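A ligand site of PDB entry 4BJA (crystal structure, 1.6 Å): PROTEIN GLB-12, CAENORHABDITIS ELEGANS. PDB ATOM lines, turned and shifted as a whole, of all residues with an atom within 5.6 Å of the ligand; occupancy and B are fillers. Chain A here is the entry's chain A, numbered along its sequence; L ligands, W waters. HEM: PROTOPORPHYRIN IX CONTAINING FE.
FE of the ligand is bound by NE2 of His 92 (2.1 Å). OG of Ser 126 sits at hydrogen-bond distance from O1A of the ligand, at 3.0 Å. A ring nitrogen (NE2) of His 127 is bound to an iron atom (FE) of the ligand. An oxygen (O2D) of the ligand is in hydrogen-bond range of the backbone NH (N) of His 92, 3.1 Å away. An oxygen (O2D) of the ligand lies close to the backbone carbonyl oxygen of Lys 88 (2.6 Å).
Water W2 lies within hydrogen-bond range of an oxygen (O1A) of the ligand (3.1 Å), the side-chain amide nitrogen (NE2) of Gln 130 (3.3 Å), the side-chain hydroxyl (OG) of Ser 126 (3.4 Å) and a ring nitrogen (ND1) of His 127 (3.4 Å). Water W1 bridges OG of Ser 126 (2.5 Å) and O1A of the ligand (3.2 Å).
Merely in contact with the ligand: Gln 130 (3.3 Å), Val 72 (3.5 Å), Leu 133 (3.5 Å), Tyr 144 (3.5 Å), Arg 95 (3.5 Å), Val 148 (3.5 Å), Met 203 (3.6 Å), Phe 96 (3.6 Å), Phe 99 (3.6 Å), Phe 73 (3.6 Å), Gly 91 (3.6 Å), Phe 145 (3.6 Å), Ile 149 (3.8 Å), Thr 123 (3.8 Å) and Leu 69 (3.9 Å). Hydrophobic or aromatic side chains within 4 Å of the ligand: Leu 69, Val 72, Phe 73, His 92, Phe 96, Phe 99, His 127, Leu 133, Tyr 144, Phe 145, Val 148, Ile 149 and Met 203. Within 4 Å of the ligand: Leu 69, Val 72, Phe 73, Lys 88, Gly 91, His 92, Arg 95, Phe 96, Phe 99, Thr 123, Ser 126, His 127, Gln 130, Leu 133, Tyr 144, Phe 145, Val 148, Ile 149 and Met 203. The nearest printed residue that does not touch the ligand is Phe 132 (4.1 Å).
The backbone carbonyl oxygen (O) of Val 72 is in hydrogen-bond range of the side-chain amino group (NZ) of Lys 88 (2.7 Å). ND1 of His 127 is in hydrogen-bond range of O of Thr 123 (2.8 Å). NH1 of Arg 95 sits close to O of Gly 91 (3.3 Å).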
ATOM      1  N   PHE A  58      -3.193  -0.660  37.972  1.00  0.00           N
ATOM      2  CA  PHE A  58      -2.096  -1.588  37.935  1.00  0.00           C
ATOM      3  C   PHE A  58      -1.947  -2.344  39.269  1.00  0.00           C
ATOM      4  O   PHE A  58      -1.572  -3.510  39.245  1.00  0.00           O
ATOM      5  CB  PHE A  58      -0.775  -0.919  37.511  1.00  0.00           C
ATOM      6  CG  PHE A  58      -0.567  -0.998  36.046  1.00  0.00           C
ATOM      7  CD1 PHE A  58      -0.170  -2.201  35.466  1.00  0.00           C
ATOM      8  CD2 PHE A  58      -0.860   0.112  35.237  1.00  0.00           C
ATOM      9  CE1 PHE A  58       0.033  -2.290  34.045  1.00  0.00           C
ATOM     10  CE2 PHE A  58      -0.672   0.018  33.832  1.00  0.00           C
ATOM     11  CZ  PHE A  58      -0.240  -1.156  33.262  1.00  0.00           C
ATOM     12  N   LEU A  69       2.262 -11.404  37.091  1.00  0.00           N
ATOM     13  CA  LEU A  69       2.930 -10.153  36.708  1.00  0.00           C
ATOM     14  C   LEU A  69       3.709  -9.509  37.830  1.00  0.00           C
ATOM     15  O   LEU A  69       4.514  -8.605  37.606  1.00  0.00           O
ATOM     16  CB  LEU A  69       1.934  -9.138  36.077  1.00  0.00           C
ATOM     17  CG  LEU A  69       1.355  -9.631  34.744  1.00  0.00           C
ATOM     18  CD1 LEU A  69       0.345  -8.597  34.214  1.00  0.00           C
ATOM     19  CD2 LEU A  69       2.455  -9.922  33.680  1.00  0.00           C
ATOM     20  N   VAL A  72       7.417 -10.032  37.258  1.00  0.00           N
ATOM     21  CA  VAL A  72       7.885  -9.294  36.085  1.00  0.00           C
ATOM     22  C   VAL A  72       8.257  -7.906  36.528  1.00  0.00           C
ATOM     23  O   VAL A  72       9.293  -7.343  36.087  1.00  0.00           O
ATOM     24  CB  VAL A  72       6.768  -9.187  34.987  1.00  0.00           C
ATOM     25  CG1 VAL A  72       7.218  -8.291  33.868  1.00  0.00           C
ATOM     26  CG2 VAL A  72       6.444 -10.530  34.453  1.00  0.00           C
ATOM     27  N   PHE A  73       7.397  -7.333  37.352  1.00  0.00           N
ATOM     28  CA  PHE A  73       7.538  -5.941  37.777  1.00  0.00           C
ATOM     29  C   PHE A  73       8.326  -5.772  39.067  1.00  0.00           C
ATOM     30  O   PHE A  73       8.377  -4.682  39.652  1.00  0.00           O
ATOM     31  CB  PHE A  73       6.167  -5.279  37.829  1.00  0.00           C
ATOM     32  CG  PHE A  73       5.578  -5.057  36.478  1.00  0.00           C
ATOM     33  CD1 PHE A  73       6.270  -4.306  35.516  1.00  0.00           C
ATOM     34  CD2 PHE A  73       4.352  -5.618  36.156  1.00  0.00           C
ATOM     35  CE1 PHE A  73       5.716  -4.110  34.226  1.00  0.00           C
ATOM     36  CE2 PHE A  73       3.790  -5.456  34.904  1.00  0.00           C
ATOM     37  CZ  PHE A  73       4.492  -4.688  33.918  1.00  0.00           C
ATOM     38  N   PRO A  87      10.873   0.169  41.331  1.00  0.00           N
ATOM     39  CA  PRO A  87      11.259   0.871  40.082  1.00  0.00           C
ATOM     40  C   PRO A  87      10.597   0.351  38.851  1.00  0.00           C
ATOM     41  O   PRO A  87      10.167   1.183  38.029  1.00  0.00           O
ATOM     42  CB  PRO A  87      12.758   0.624  39.969  1.00  0.00           C
ATOM     43  CG  PRO A  87      13.183   0.006  41.235  1.00  0.00           C
ATOM     44  CD  PRO A  87      12.028  -0.345  42.095  1.00  0.00           C
ATOM     45  N   LYS A  88      10.552  -0.970  38.664  1.00  0.00           N
ATOM     46  CA  LYS A  88       9.959  -1.491  37.397  1.00  0.00           C
ATOM     47  C   LYS A  88       8.461  -1.264  37.403  1.00  0.00           C
ATOM     48  O   LYS A  88       7.864  -0.952  36.364  1.00  0.00           O
ATOM     49  CB  LYS A  88      10.250  -2.979  37.192  1.00  0.00           C
ATOM     50  CG  LYS A  88      11.717  -3.349  37.014  1.00  0.00           C
ATOM     51  CD  LYS A  88      11.919  -4.779  36.447  1.00  0.00           C
ATOM     52  CE  LYS A  88      11.281  -4.997  35.028  1.00  0.00           C
ATOM     53  NZ  LYS A  88      11.302  -6.470  34.574  1.00  0.00           N
ATOM     54  N   PHE A  89       7.850  -1.391  38.583  1.00  0.00           N
ATOM     55  CA  PHE A  89       6.374  -1.248  38.682  1.00  0.00           C
ATOM     56  C   PHE A  89       5.919   0.220  38.578  1.00  0.00           C
ATOM     57  O   PHE A  89       5.079   0.565  37.721  1.00  0.00           O
ATOM     58  CB  PHE A  89       5.888  -1.921  39.962  1.00  0.00           C
ATOM     59  CG  PHE A  89       4.369  -1.928  40.076  1.00  0.00           C
ATOM     60  CD1 PHE A  89       3.592  -2.805  39.308  1.00  0.00           C
ATOM     61  CD2 PHE A  89       3.731  -1.030  40.933  1.00  0.00           C
ATOM     62  CE1 PHE A  89       2.162  -2.794  39.449  1.00  0.00           C
ATOM     63  CE2 PHE A  89       2.331  -1.012  41.091  1.00  0.00           C
ATOM     64  CZ  PHE A  89       1.553  -1.873  40.308  1.00  0.00           C
ATOM     65  N   GLY A  91       7.685   2.459  37.410  1.00  0.00           N
ATOM     66  CA  GLY A  91       8.177   2.922  36.071  1.00  0.00           C
ATOM     67  C   GLY A  91       7.123   2.608  35.019  1.00  0.00           C
ATOM     68  O   GLY A  91       6.859   3.409  34.101  1.00  0.00           O
ATOM     69  N   HIS A  92       6.533   1.432  35.150  1.00  0.00           N
ATOM     70  CA  HIS A  92       5.564   1.022  34.156  1.00  0.00           C
ATOM     71  C   HIS A  92       4.306   1.874  34.226  1.00  0.00           C
ATOM     72  O   HIS A  92       3.677   2.140  33.191  1.00  0.00           O
ATOM     73  CB  HIS A  92       5.217  -0.437  34.289  1.00  0.00           C
ATOM     74  CG  HIS A  92       4.634  -0.980  33.036  1.00  0.00           C
ATOM     75  ND1 HIS A  92       3.281  -1.185  32.867  1.00  0.00           N
ATOM     76  CD2 HIS A  92       5.207  -1.270  31.836  1.00  0.00           C
ATOM     77  CE1 HIS A  92       3.055  -1.628  31.644  1.00  0.00           C
ATOM     78  NE2 HIS A  92       4.200  -1.682  30.995  1.00  0.00           N
ATOM     79  N   ARG A  95       5.058   5.042  32.488  1.00  0.00           N
ATOM     80  CA  ARG A  95       5.170   4.831  31.016  1.00  0.00           C
ATOM     81  C   ARG A  95       3.801   4.660  30.393  1.00  0.00           C
ATOM     82  O   ARG A  95       3.527   5.208  29.299  1.00  0.00           O
ATOM     83  CB  ARG A  95       6.065   3.623  30.674  1.00  0.00           C
ATOM     84  CG  ARG A  95       7.569   3.867  30.989  1.00  0.00           C
ATOM     85  CD  ARG A  95       8.311   2.551  31.157  1.00  0.00           C
ATOM     86  NE  ARG A  95       9.792   2.635  31.108  1.00  0.00           N
ATOM     87  CZ  ARG A  95      10.559   3.016  32.125  1.00  0.00           C
ATOM     88  NH1 ARG A  95      10.014   3.403  33.277  1.00  0.00           N
ATOM     89  NH2 ARG A  95      11.887   3.034  31.988  1.00  0.00           N
ATOM     90  N   PHE A  96       2.942   3.901  31.068  1.00  0.00           N
ATOM     91  CA  PHE A  96       1.590   3.618  30.568  1.00  0.00           C
ATOM     92  C   PHE A  96       0.762   4.888  30.616  1.00  0.00           C
ATOM     93  O   PHE A  96       0.104   5.242  29.661  1.00  0.00           O
ATOM     94  CB  PHE A  96       0.947   2.501  31.414  1.00  0.00           C
ATOM     95  CG  PHE A  96      -0.375   2.068  30.921  1.00  0.00           C
ATOM     96  CD1 PHE A  96      -1.499   2.806  31.201  1.00  0.00           C
ATOM     97  CD2 PHE A  96      -0.489   0.888  30.203  1.00  0.00           C
ATOM     98  CE1 PHE A  96      -2.754   2.414  30.714  1.00  0.00           C
ATOM     99  CE2 PHE A  96      -1.743   0.467  29.696  1.00  0.00           C
ATOM    100  CZ  PHE A  96      -2.878   1.239  29.983  1.00  0.00           C
ATOM    101  N   PHE A  99       1.987   7.110  27.785  1.00  0.00           N
ATOM    102  CA  PHE A  99       1.513   6.532  26.514  1.00  0.00           C
ATOM    103  C   PHE A  99       0.061   6.926  26.269  1.00  0.00           C
ATOM    104  O   PHE A  99      -0.273   7.323  25.157  1.00  0.00           O
ATOM    105  CB  PHE A  99       1.678   5.022  26.593  1.00  0.00           C
ATOM    106  CG  PHE A  99       0.971   4.229  25.524  1.00  0.00           C
ATOM    107  CD1 PHE A  99      -0.341   3.797  25.692  1.00  0.00           C
ATOM    108  CD2 PHE A  99       1.681   3.832  24.384  1.00  0.00           C
ATOM    109  CE1 PHE A  99      -0.968   3.018  24.720  1.00  0.00           C
ATOM    110  CE2 PHE A  99       1.073   3.025  23.425  1.00  0.00           C
ATOM    111  CZ  PHE A  99      -0.257   2.638  23.579  1.00  0.00           C
ATOM    112  N   LYS A 122       4.807   0.679  17.669  1.00  0.00           N
ATOM    113  CA  LYS A 122       6.181   0.736  18.145  1.00  0.00           C
ATOM    114  C   LYS A 122       6.244   0.161  19.562  1.00  0.00           C
ATOM    115  O   LYS A 122       7.222  -0.519  19.944  1.00  0.00           O
ATOM    116  CB  LYS A 122       6.723   2.189  18.183  1.00  0.00           C
ATOM    117  CG  LYS A 122       8.145   2.236  18.725  1.00  0.00           C
ATOM    118  CD  LYS A 122       8.790   3.597  18.584  1.00  0.00           C
ATOM    119  CE  LYS A 122      10.270   3.540  19.087  1.00  0.00           C
ATOM    120  NZ  LYS A 122      10.969   4.813  18.878  1.00  0.00           N
ATOM    121  N   THR A 123       5.211   0.479  20.334  1.00  0.00           N
ATOM    122  CA  THR A 123       5.149   0.007  21.734  1.00  0.00           C
ATOM    123  C   THR A 123       4.944  -1.495  21.739  1.00  0.00           C
ATOM    124  O   THR A 123       5.593  -2.218  22.499  1.00  0.00           O
ATOM    125  CB  THR A 123       4.055   0.780  22.486  1.00  0.00           C
ATOM    126  OG1 THR A 123       4.343   2.183  22.418  1.00  0.00           O
ATOM    127  CG2 THR A 123       3.942   0.398  23.981  1.00  0.00           C
ATOM    128  N   SER A 126       8.190  -3.171  20.885  1.00  0.00           N
ATOM    129  CA  SER A 126       9.214  -2.997  21.886  1.00  0.00           C
ATOM    130  C   SER A 126       9.068  -4.002  23.003  1.00  0.00           C
ATOM    131  O   SER A 126      10.048  -4.339  23.703  1.00  0.00           O
ATOM    132  CB  SER A 126       9.157  -1.590  22.460  1.00  0.00           C
ATOM    133  OG  SER A 126       9.860  -1.550  23.685  1.00  0.00           O
ATOM    134  N   HIS A 127       7.857  -4.486  23.190  1.00  0.00           N
ATOM    135  CA  HIS A 127       7.625  -5.469  24.272  1.00  0.00           C
ATOM    136  C   HIS A 127       8.212  -6.826  24.003  1.00  0.00           C
ATOM    137  O   HIS A 127       8.265  -7.662  24.909  1.00  0.00           O
ATOM    138  CB  HIS A 127       6.103  -5.528  24.624  1.00  0.00           C
ATOM    139  CG  HIS A 127       5.672  -4.413  25.544  1.00  0.00           C
ATOM    140  ND1 HIS A 127       5.481  -3.120  25.111  1.00  0.00           N
ATOM    141  CD2 HIS A 127       5.418  -4.402  26.873  1.00  0.00           C
ATOM    142  CE1 HIS A 127       5.124  -2.367  26.139  1.00  0.00           C
ATOM    143  NE2 HIS A 127       5.093  -3.118  27.216  1.00  0.00           N
ATOM    144  N   GLN A 130      10.864  -7.992  26.351  1.00  0.00           N
ATOM    145  CA  GLN A 130      10.485  -8.502  27.665  1.00  0.00           C
ATOM    146  C   GLN A 130      10.416  -9.994  27.591  1.00  0.00           C
ATOM    147  O   GLN A 130       9.556 -10.551  26.931  1.00  0.00           O
ATOM    148  CB  GLN A 130       9.145  -7.921  28.143  1.00  0.00           C
ATOM    149  CG  GLN A 130       9.084  -6.389  28.230  1.00  0.00           C
ATOM    150  CD  GLN A 130      10.277  -5.749  28.938  1.00  0.00           C
ATOM    151  OE1 GLN A 130      10.893  -6.359  29.805  1.00  0.00           O
ATOM    152  NE2 GLN A 130      10.584  -4.492  28.587  1.00  0.00           N
ATOM    153  N   PHE A 132       9.530 -12.341  29.571  1.00  0.00           N
ATOM    154  CA  PHE A 132       8.313 -12.956  30.053  1.00  0.00           C
ATOM    155  C   PHE A 132       7.299 -12.960  28.918  1.00  0.00           C
ATOM    156  O   PHE A 132       6.628 -13.945  28.668  1.00  0.00           O
ATOM    157  CB  PHE A 132       7.728 -12.216  31.249  1.00  0.00           C
ATOM    158  CG  PHE A 132       6.380 -12.712  31.657  1.00  0.00           C
ATOM    159  CD1 PHE A 132       6.244 -13.780  32.561  1.00  0.00           C
ATOM    160  CD2 PHE A 132       5.214 -12.111  31.163  1.00  0.00           C
ATOM    161  CE1 PHE A 132       4.958 -14.237  32.933  1.00  0.00           C
ATOM    162  CE2 PHE A 132       3.955 -12.561  31.524  1.00  0.00           C
ATOM    163  CZ  PHE A 132       3.823 -13.658  32.421  1.00  0.00           C
ATOM    164  N   LEU A 133       7.199 -11.835  28.216  1.00  0.00           N
ATOM    165  CA  LEU A 133       6.207 -11.780  27.133  1.00  0.00           C
ATOM    166  C   LEU A 133       6.663 -12.579  25.917  1.00  0.00           C
ATOM    167  O   LEU A 133       5.847 -13.233  25.283  1.00  0.00           O
ATOM    168  CB  LEU A 133       5.915 -10.324  26.749  1.00  0.00           C
ATOM    169  CG  LEU A 133       5.144  -9.514  27.786  1.00  0.00           C
ATOM    170  CD1 LEU A 133       5.095  -8.053  27.340  1.00  0.00           C
ATOM    171  CD2 LEU A 133       3.694 -10.051  27.936  1.00  0.00           C
ATOM    172  N   TYR A 144      -1.471 -10.987  27.217  1.00  0.00           N
ATOM    173  CA  TYR A 144      -1.252 -10.113  28.372  1.00  0.00           C
ATOM    174  C   TYR A 144      -1.621  -8.655  28.075  1.00  0.00           C
ATOM    175  O   TYR A 144      -1.959  -7.927  28.974  1.00  0.00           O
ATOM    176  CB  TYR A 144       0.206 -10.239  28.908  1.00  0.00           C
ATOM    177  CG  TYR A 144       0.448 -11.602  29.509  1.00  0.00           C
ATOM    178  CD1 TYR A 144       0.128 -11.857  30.838  1.00  0.00           C
ATOM    179  CD2 TYR A 144       0.968 -12.626  28.733  1.00  0.00           C
ATOM    180  CE1 TYR A 144       0.350 -13.119  31.374  1.00  0.00           C
ATOM    181  CE2 TYR A 144       1.177 -13.888  29.263  1.00  0.00           C
ATOM    182  CZ  TYR A 144       0.851 -14.115  30.571  1.00  0.00           C
ATOM    183  OH  TYR A 144       1.072 -15.377  31.093  1.00  0.00           O
ATOM    184  N   PHE A 145      -1.574  -8.220  26.799  1.00  0.00           N
ATOM    185  CA  PHE A 145      -2.029  -6.883  26.507  1.00  0.00           C
ATOM    186  C   PHE A 145      -3.527  -6.802  26.709  1.00  0.00           C
ATOM    187  O   PHE A 145      -4.038  -5.807  27.257  1.00  0.00           O
ATOM    188  CB  PHE A 145      -1.699  -6.528  25.046  1.00  0.00           C
ATOM    189  CG  PHE A 145      -0.233  -6.624  24.740  1.00  0.00           C
ATOM    190  CD1 PHE A 145       0.702  -5.964  25.561  1.00  0.00           C
ATOM    191  CD2 PHE A 145       0.212  -7.441  23.689  1.00  0.00           C
ATOM    192  CE1 PHE A 145       2.073  -6.072  25.259  1.00  0.00           C
ATOM    193  CE2 PHE A 145       1.558  -7.554  23.412  1.00  0.00           C
ATOM    194  CZ  PHE A 145       2.492  -6.873  24.196  1.00  0.00           C
ATOM    195  N   GLU A 146      -4.219  -7.866  26.300  1.00  0.00           N
ATOM    196  CA  GLU A 146      -5.639  -7.934  26.505  1.00  0.00           C
ATOM    197  C   GLU A 146      -5.992  -8.016  28.025  1.00  0.00           C
ATOM    198  O   GLU A 146      -6.888  -7.331  28.510  1.00  0.00           O
ATOM    199  CB  GLU A 146      -6.181  -9.140  25.742  1.00  0.00           C
ATOM    200  CG  GLU A 146      -7.677  -9.291  25.879  1.00  0.00           C
ATOM    201  CD  GLU A 146      -8.135 -10.519  25.136  1.00  0.00           C
ATOM    202  OE1 GLU A 146      -7.950 -11.625  25.665  1.00  0.00           O
ATOM    203  OE2 GLU A 146      -8.640 -10.394  23.999  1.00  0.00           O
ATOM    204  N   VAL A 148      -4.341  -6.842  30.569  1.00  0.00           N
ATOM    205  CA  VAL A 148      -4.128  -5.548  31.216  1.00  0.00           C
ATOM    206  C   VAL A 148      -5.203  -4.568  30.801  1.00  0.00           C
ATOM    207  O   VAL A 148      -5.823  -3.867  31.639  1.00  0.00           O
ATOM    208  CB  VAL A 148      -2.714  -4.998  30.849  1.00  0.00           C
ATOM    209  CG1 VAL A 148      -2.559  -3.549  31.256  1.00  0.00           C
ATOM    210  CG2 VAL A 148      -1.606  -5.866  31.556  1.00  0.00           C
ATOM    211  N   ILE A 149      -5.395  -4.430  29.481  1.00  0.00           N
ATOM    212  CA  ILE A 149      -6.335  -3.406  29.000  1.00  0.00           C
ATOM    213  C   ILE A 149      -7.761  -3.752  29.405  1.00  0.00           C
ATOM    214  O   ILE A 149      -8.527  -2.857  29.692  1.00  0.00           O
ATOM    215  CB  ILE A 149      -6.205  -3.139  27.506  1.00  0.00           C
ATOM    216  CG1 ILE A 149      -4.843  -2.510  27.307  1.00  0.00           C
ATOM    217  CG2 ILE A 149      -7.374  -2.231  27.025  1.00  0.00           C
ATOM    218  CD1 ILE A 149      -4.764  -1.089  27.765  1.00  0.00           C
ATOM    219  N   VAL A 199      -6.301  -0.481  20.737  1.00  0.00           N
ATOM    220  CA  VAL A 199      -4.960  -0.532  21.290  1.00  0.00           C
ATOM    221  C   VAL A 199      -4.522  -1.986  21.502  1.00  0.00           C
ATOM    222  O   VAL A 199      -3.426  -2.403  21.117  1.00  0.00           O
ATOM    223  CB  VAL A 199      -4.876   0.271  22.597  1.00  0.00           C
ATOM    224  CG1 VAL A 199      -3.522   0.016  23.269  1.00  0.00           C
ATOM    225  CG2 VAL A 199      -5.104   1.810  22.275  1.00  0.00           C
ATOM    226  N   MET A 203      -1.324  -3.544  19.440  1.00  0.00           N
ATOM    227  CA  MET A 203      -0.155  -4.000  20.187  1.00  0.00           C
ATOM    228  C   MET A 203       0.028  -5.488  20.015  1.00  0.00           C
ATOM    229  O   MET A 203       1.156  -5.939  19.855  1.00  0.00           O
ATOM    230  CB  MET A 203      -0.235  -3.638  21.652  1.00  0.00           C
ATOM    231  CG  MET A 203      -0.089  -2.159  21.867  1.00  0.00           C
ATOM    232  SD  MET A 203      -0.279  -1.814  23.600  1.00  0.00           S
ATOM    233  CE  MET A 203       1.290  -2.382  24.214  1.00  0.00           C
HETATM  234  CHA HEM L   1       7.697  -0.894  28.931  1.00  0.00           C
HETATM  235  CHB HEM L   1       3.185   0.431  27.762  1.00  0.00           C
HETATM  236  CHC HEM L   1       1.620  -4.013  28.739  1.00  0.00           C
HETATM  237  CHD HEM L   1       5.917  -5.076  30.651  1.00  0.00           C
HETATM  238  C1A HEM L   1       6.626  -0.198  28.481  1.00  0.00           C
HETATM  239  C2A HEM L   1       6.676   1.139  27.921  1.00  0.00           C
HETATM  240  C3A HEM L   1       5.410   1.473  27.607  1.00  0.00           C
HETATM  241  C4A HEM L   1       4.546   0.383  27.972  1.00  0.00           C
HETATM  242  CMA HEM L   1       4.891   2.795  26.988  1.00  0.00           C
HETATM  243  CAA HEM L   1       7.987   1.957  27.707  1.00  0.00           C
HETATM  244  CBA HEM L   1       8.237   2.254  26.221  1.00  0.00           C
HETATM  245  CGA HEM L   1       8.402   0.960  25.540  1.00  0.00           C
HETATM  246  O1A HEM L   1       9.196   0.127  26.046  1.00  0.00           O
HETATM  247  O2A HEM L   1       7.688   0.793  24.519  1.00  0.00           O
HETATM  248  C1B HEM L   1       2.422  -0.695  27.881  1.00  0.00           C
HETATM  249  C2B HEM L   1       1.038  -0.803  27.429  1.00  0.00           C
HETATM  250  C3B HEM L   1       0.619  -2.016  27.685  1.00  0.00           C
HETATM  251  C4B HEM L   1       1.698  -2.724  28.327  1.00  0.00           C
HETATM  252  CMB HEM L   1       0.237   0.320  26.739  1.00  0.00           C
HETATM  253  CAB HEM L   1      -0.797  -2.544  27.318  1.00  0.00           C
HETATM  254  CBB HEM L   1      -1.273  -3.574  27.959  1.00  0.00           C
HETATM  255  C1C HEM L   1       2.640  -4.676  29.323  1.00  0.00           C
HETATM  256  C2C HEM L   1       2.566  -6.038  29.815  1.00  0.00           C
HETATM  257  C3C HEM L   1       3.751  -6.338  30.328  1.00  0.00           C
HETATM  258  C4C HEM L   1       4.601  -5.178  30.219  1.00  0.00           C
HETATM  259  CMC HEM L   1       1.329  -6.952  29.688  1.00  0.00           C
HETATM  260  CAC HEM L   1       4.103  -7.707  30.960  1.00  0.00           C
HETATM  261  CBC HEM L   1       5.376  -8.061  30.959  1.00  0.00           C
HETATM  262  C1D HEM L   1       6.739  -4.028  30.434  1.00  0.00           C
HETATM  263  C2D HEM L   1       8.045  -3.888  31.008  1.00  0.00           C
HETATM  264  C3D HEM L   1       8.587  -2.606  30.474  1.00  0.00           C
HETATM  265  C4D HEM L   1       7.569  -2.077  29.610  1.00  0.00           C
HETATM  266  CMD HEM L   1       8.768  -4.830  31.994  1.00  0.00           C
HETATM  267  CAD HEM L   1       9.950  -1.958  30.815  1.00  0.00           C
HETATM  268  CBD HEM L   1       9.657  -0.835  31.827  1.00  0.00           C
HETATM  269  CGD HEM L   1       9.207  -1.314  33.212  1.00  0.00           C
HETATM  270  O1D HEM L   1       9.472  -2.463  33.612  1.00  0.00           O
HETATM  271  O2D HEM L   1       8.588  -0.506  33.905  1.00  0.00           O
HETATM  272  NA  HEM L   1       5.300  -0.634  28.522  1.00  0.00           N
HETATM  273  NB  HEM L   1       2.819  -1.903  28.440  1.00  0.00           N
HETATM  274  NC  HEM L   1       3.902  -4.197  29.600  1.00  0.00           N
HETATM  275  ND  HEM L   1       6.485  -2.930  29.607  1.00  0.00           N
HETATM  276 FE   HEM L   1       4.640  -2.395  29.060  1.00  0.00          FE
HETATM  277  O   HOH W   1      11.535  -2.013  25.458  1.00  0.00           O
HETATM  278  O   HOH W   2       8.571  -2.907  26.493  1.00  0.00           O
